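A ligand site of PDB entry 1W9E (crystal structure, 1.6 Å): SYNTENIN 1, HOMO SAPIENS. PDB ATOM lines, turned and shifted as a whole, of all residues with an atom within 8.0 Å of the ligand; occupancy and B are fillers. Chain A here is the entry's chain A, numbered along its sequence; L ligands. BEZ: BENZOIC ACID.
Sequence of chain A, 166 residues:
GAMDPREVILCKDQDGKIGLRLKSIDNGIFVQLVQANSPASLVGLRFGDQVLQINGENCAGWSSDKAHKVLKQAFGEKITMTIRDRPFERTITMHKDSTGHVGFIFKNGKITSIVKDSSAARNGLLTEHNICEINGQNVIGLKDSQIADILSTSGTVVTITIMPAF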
ATOM      1  N   ILE A  92      14.673 -17.725   3.212  1.00  0.00           N
ATOM      2  CA  ILE A  92      13.712 -18.616   2.578  1.00  0.00           C
ATOM      3  C   ILE A  92      12.323 -18.016   2.760  1.00  0.00           C
ATOM      4  O   ILE A  92      11.965 -17.614   3.851  1.00  0.00           O
ATOM      5  CB  ILE A  92      13.741 -20.019   3.237  1.00  0.00           C
ATOM      6  CG1 ILE A  92      15.068 -20.738   2.958  1.00  0.00           C
ATOM      7  CG2 ILE A  92      12.583 -20.900   2.680  1.00  0.00           C
ATOM      8  CD1 ILE A  92      15.114 -21.448   1.575  1.00  0.00           C
ATOM      9  N   THR A  93      11.564 -17.975   1.669  1.00  0.00           N
ATOM     10  CA  THR A  93      10.187 -17.496   1.692  1.00  0.00           C
ATOM     11  C   THR A  93       9.235 -18.657   1.406  1.00  0.00           C
ATOM     12  O   THR A  93       9.422 -19.407   0.454  1.00  0.00           O
ATOM     13  CB  THR A  93      10.047 -16.394   0.658  1.00  0.00           C
ATOM     14  OG1 THR A  93      10.912 -15.302   1.008  1.00  0.00           O
ATOM     15  CG2 THR A  93       8.655 -15.829   0.672  1.00  0.00           C
ATOM     16  N   MET A  94       8.230 -18.784   2.253  1.00  0.00           N
ATOM     17  CA  MET A  94       7.223 -19.816   2.154  1.00  0.00           C
ATOM     18  C   MET A  94       5.840 -19.178   2.196  1.00  0.00           C
ATOM     19  O   MET A  94       5.701 -18.016   2.529  1.00  0.00           O
ATOM     20  CB  MET A  94       7.360 -20.814   3.300  1.00  0.00           C
ATOM     21  CG  MET A  94       8.655 -21.619   3.251  1.00  0.00           C
ATOM     22  SD  MET A  94       9.102 -22.378   4.829  1.00  0.00           S
ATOM     23  CE  MET A  94       9.697 -20.969   5.761  1.00  0.00           C
ATOM     24  N   HIS A  95       4.850 -19.955   1.787  1.00  0.00           N
ATOM     25  CA  HIS A  95       3.449 -19.552   1.825  1.00  0.00           C
ATOM     26  C   HIS A  95       2.663 -20.504   2.678  1.00  0.00           C
ATOM     27  O   HIS A  95       2.796 -21.726   2.546  1.00  0.00           O
ATOM     28  CB  HIS A  95       2.807 -19.619   0.456  1.00  0.00           C
ATOM     29  CG  HIS A  95       3.208 -18.533  -0.506  1.00  0.00           C
ATOM     30  ND1 HIS A  95       4.481 -18.024  -0.621  1.00  0.00           N
ATOM     31  CD2 HIS A  95       2.456 -17.871  -1.411  1.00  0.00           C
ATOM     32  CE1 HIS A  95       4.499 -17.095  -1.569  1.00  0.00           C
ATOM     33  NE2 HIS A  95       3.278 -16.968  -2.045  1.00  0.00           N
ATOM     34  N   LYS A  96       1.881 -19.978   3.610  1.00  0.00           N
ATOM     35  CA  LYS A  96       0.969 -20.810   4.366  1.00  0.00           C
ATOM     36  C   LYS A  96      -0.027 -21.502   3.450  1.00  0.00           C
ATOM     37  O   LYS A  96      -0.480 -20.915   2.461  1.00  0.00           O
ATOM     38  CB  LYS A  96       0.166 -19.963   5.344  1.00  0.00           C
ATOM     39  CG  LYS A  96       1.002 -19.392   6.478  1.00  0.00           C
ATOM     40  CD  LYS A  96       0.150 -18.553   7.405  1.00  0.00           C
ATOM     41  CE  LYS A  96       0.953 -18.135   8.634  1.00  0.00           C
ATOM     42  NZ  LYS A  96       0.102 -17.415   9.687  1.00  0.00           N
ATOM     43  N   ASP A  97      -0.350 -22.725   3.805  1.00  0.00           N
ATOM     44  CA  ASP A  97      -1.358 -23.523   3.074  1.00  0.00           C
ATOM     45  C   ASP A  97      -2.739 -23.233   3.639  1.00  0.00           C
ATOM     46  O   ASP A  97      -2.896 -22.318   4.429  1.00  0.00           O
ATOM     47  CB  ASP A  97      -1.007 -25.021   3.074  1.00  0.00           C
ATOM     48  CG  ASP A  97      -1.096 -25.682   4.447  1.00  0.00           C
ATOM     49  OD1 ASP A  97      -1.701 -25.122   5.392  1.00  0.00           O
ATOM     50  OD2 ASP A  97      -0.558 -26.809   4.661  1.00  0.00           O
ATOM     51  N   VAL A 102       3.117 -23.465   7.047  1.00  0.00           N
ATOM     52  CA  VAL A 102       4.153 -23.431   6.011  1.00  0.00           C
ATOM     53  C   VAL A 102       4.859 -24.777   5.840  1.00  0.00           C
ATOM     54  O   VAL A 102       5.414 -25.032   4.755  1.00  0.00           O
ATOM     55  CB  VAL A 102       5.195 -22.305   6.247  1.00  0.00           C
ATOM     56  CG1 VAL A 102       4.516 -20.965   6.198  1.00  0.00           C
ATOM     57  CG2 VAL A 102       5.970 -22.521   7.527  1.00  0.00           C
ATOM     58  N   ASP A 117       5.296 -32.215   1.059  1.00  0.00           N
ATOM     59  CA  ASP A 117       4.581 -31.443   0.053  1.00  0.00           C
ATOM     60  C   ASP A 117       4.009 -30.115   0.530  1.00  0.00           C
ATOM     61  O   ASP A 117       3.141 -29.525  -0.088  1.00  0.00           O
ATOM     62  CB  ASP A 117       3.574 -32.299  -0.690  1.00  0.00           C
ATOM     63  CG  ASP A 117       4.206 -33.529  -1.348  1.00  0.00           C
ATOM     64  OD1 ASP A 117       5.393 -33.537  -1.826  1.00  0.00           O
ATOM     65  OD2 ASP A 117       3.564 -34.568  -1.446  1.00  0.00           O
ATOM     66  N   SER A 118       4.619 -29.602   1.583  1.00  0.00           N
ATOM     67  CA  SER A 118       4.375 -28.264   2.054  1.00  0.00           C
ATOM     68  C   SER A 118       5.217 -27.231   1.312  1.00  0.00           C
ATOM     69  O   SER A 118       6.073 -27.557   0.503  1.00  0.00           O
ATOM     70  CB  SER A 118       4.733 -28.194   3.553  1.00  0.00           C
ATOM     71  OG  SER A 118       6.128 -28.416   3.695  1.00  0.00           O
ATOM     72  N   SER A 119       4.935 -25.975   1.588  1.00  0.00           N
ATOM     73  CA  SER A 119       5.719 -24.899   1.030  1.00  0.00           C
ATOM     74  C   SER A 119       7.183 -25.018   1.540  1.00  0.00           C
ATOM     75  O   SER A 119       8.118 -24.786   0.772  1.00  0.00           O
ATOM     76  CB  SER A 119       5.119 -23.547   1.403  1.00  0.00           C
ATOM     77  OG  SER A 119       5.880 -22.497   0.822  1.00  0.00           O
ATOM     78  N   ALA A 120       7.381 -25.359   2.787  1.00  0.00           N
ATOM     79  CA  ALA A 120       8.733 -25.620   3.259  1.00  0.00           C
ATOM     80  C   ALA A 120       9.461 -26.678   2.406  1.00  0.00           C
ATOM     81  O   ALA A 120      10.616 -26.551   2.082  1.00  0.00           O
ATOM     82  CB  ALA A 120       8.763 -25.999   4.737  1.00  0.00           C
ATOM     83  N   ALA A 121       8.776 -27.764   2.111  1.00  0.00           N
ATOM     84  CA  ALA A 121       9.338 -28.789   1.232  1.00  0.00           C
ATOM     85  C   ALA A 121       9.640 -28.256  -0.144  1.00  0.00           C
ATOM     86  O   ALA A 121      10.759 -28.448  -0.665  1.00  0.00           O
ATOM     87  CB  ALA A 121       8.415 -29.941   1.113  1.00  0.00           C
ATOM     88  N   ARG A 122       8.685 -27.571  -0.755  1.00  0.00           N
ATOM     89  CA  ARG A 122       8.924 -27.041  -2.109  1.00  0.00           C
ATOM     90  C   ARG A 122      10.093 -26.097  -2.178  1.00  0.00           C
ATOM     91  O   ARG A 122      10.792 -26.048  -3.174  1.00  0.00           O
ATOM     92  CB  ARG A 122       7.678 -26.375  -2.689  1.00  0.00           C
ATOM     93  CG  ARG A 122       6.533 -27.308  -3.016  1.00  0.00           C
ATOM     94  CD  ARG A 122       5.426 -26.566  -3.766  1.00  0.00           C
ATOM     95  NE  ARG A 122       4.811 -25.486  -3.003  1.00  0.00           N
ATOM     96  CZ  ARG A 122       3.835 -25.653  -2.099  1.00  0.00           C
ATOM     97  NH1 ARG A 122       3.349 -26.846  -1.811  1.00  0.00           N
ATOM     98  NH2 ARG A 122       3.330 -24.585  -1.466  1.00  0.00           N
ATOM     99  N   ASN A 123      10.262 -25.293  -1.119  1.00  0.00           N
ATOM    100  CA  ASN A 123      11.353 -24.317  -1.041  1.00  0.00           C
ATOM    101  C   ASN A 123      12.661 -24.887  -0.526  1.00  0.00           C
ATOM    102  O   ASN A 123      13.646 -24.179  -0.442  1.00  0.00           O
ATOM    103  CB  ASN A 123      10.907 -23.145  -0.168  1.00  0.00           C
ATOM    104  CG  ASN A 123       9.965 -22.197  -0.912  1.00  0.00           C
ATOM    105  OD1 ASN A 123      10.396 -21.333  -1.690  1.00  0.00           O
ATOM    106  ND2 ASN A 123       8.686 -22.407  -0.743  1.00  0.00           N
ATOM    107  N   THR A 156       0.029 -14.769   4.865  1.00  0.00           N
ATOM    108  CA  THR A 156       0.293 -15.983   4.140  1.00  0.00           C
ATOM    109  C   THR A 156       1.806 -16.099   3.814  1.00  0.00           C
ATOM    110  O   THR A 156       2.392 -17.176   3.917  1.00  0.00           O
ATOM    111  CB  THR A 156      -0.505 -15.959   2.884  1.00  0.00           C
ATOM    112  OG1 THR A 156      -1.924 -15.946   3.217  1.00  0.00           O
ATOM    113  CG2 THR A 156      -0.254 -17.201   2.009  1.00  0.00           C
ATOM    114  N   VAL A 157       2.400 -14.991   3.399  1.00  0.00           N
ATOM    115  CA  VAL A 157       3.791 -15.035   2.960  1.00  0.00           C
ATOM    116  C   VAL A 157       4.687 -14.848   4.198  1.00  0.00           C
ATOM    117  O   VAL A 157       4.551 -13.882   4.960  1.00  0.00           O
ATOM    118  CB  VAL A 157       4.088 -14.039   1.836  1.00  0.00           C
ATOM    119  CG1 VAL A 157       5.567 -14.155   1.425  1.00  0.00           C
ATOM    120  CG2 VAL A 157       3.183 -14.269   0.624  1.00  0.00           C
ATOM    121  N   VAL A 158       5.580 -15.803   4.393  1.00  0.00           N
ATOM    122  CA  VAL A 158       6.415 -15.891   5.577  1.00  0.00           C
ATOM    123  C   VAL A 158       7.855 -15.966   5.107  1.00  0.00           C
ATOM    124  O   VAL A 158       8.253 -16.936   4.480  1.00  0.00           O
ATOM    125  CB  VAL A 158       6.077 -17.155   6.401  1.00  0.00           C
ATOM    126  CG1 VAL A 158       6.989 -17.307   7.630  1.00  0.00           C
ATOM    127  CG2 VAL A 158       4.599 -17.147   6.840  1.00  0.00           C
HETATM  128  C   BEZ L   1       5.196 -21.193  -2.244  1.00  0.00           C
HETATM  129  O1  BEZ L   1       6.502 -20.733  -2.108  1.00  0.00           O
HETATM  130  O2  BEZ L   1       4.884 -22.260  -1.583  1.00  0.00           O
HETATM  131  C1  BEZ L   1       4.199 -20.535  -3.143  1.00  0.00           C
HETATM  132  C2  BEZ L   1       2.853 -20.907  -3.108  1.00  0.00           C
HETATM  133  C3  BEZ L   1       1.938 -20.278  -3.953  1.00  0.00           C
HETATM  134  C4  BEZ L   1       2.379 -19.282  -4.840  1.00  0.00           C
HETATM  135  C5  BEZ L   1       3.721 -18.928  -4.868  1.00  0.00           C
HETATM  136  C6  BEZ L   1       4.628 -19.543  -4.018  1.00  0.00           C
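O2 of the ligand sits at hydrogen-bond distance from OG of Ser 119, at 2.6 Å.
O2 of the ligand lies within salt-bridge range of NH2 of Arg 122, 2.8 Å away.
The side-chain amide nitrogen (ND2) of Asn 123 is in hydrogen-bond range of an oxygen (O1) of the ligand, 3.1 Å away.
The backbone carbonyl oxygen of Ser 119 is in hydrogen-bond range of the side-chain amide nitrogen of Asn 123 (2.9 Å).
The side-chain hydroxyl (OG) of Ser 119 is in hydrogen-bond range of the backbone NH (N) of His 95, at 2.9 Å.
N of Ser 119 is in hydrogen-bond range of O of Val 102, at 3.3 Å.
NH1 of Arg 122 sits at hydrogen-bond distance from O of Asp 117 (3.2 Å).
The side-chain amide oxygen of Asn 123 lies close to the backbone carbonyl oxygen of Thr 93, 3.0 Å away.
His 95 touches the ligand.
Hydrophobic or aromatic side chains within 4 Å of the ligand: His 95.
Four residues have an atom within 4 Å of the ligand: His 95, Ser 119, Arg 122 and Asn 123.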
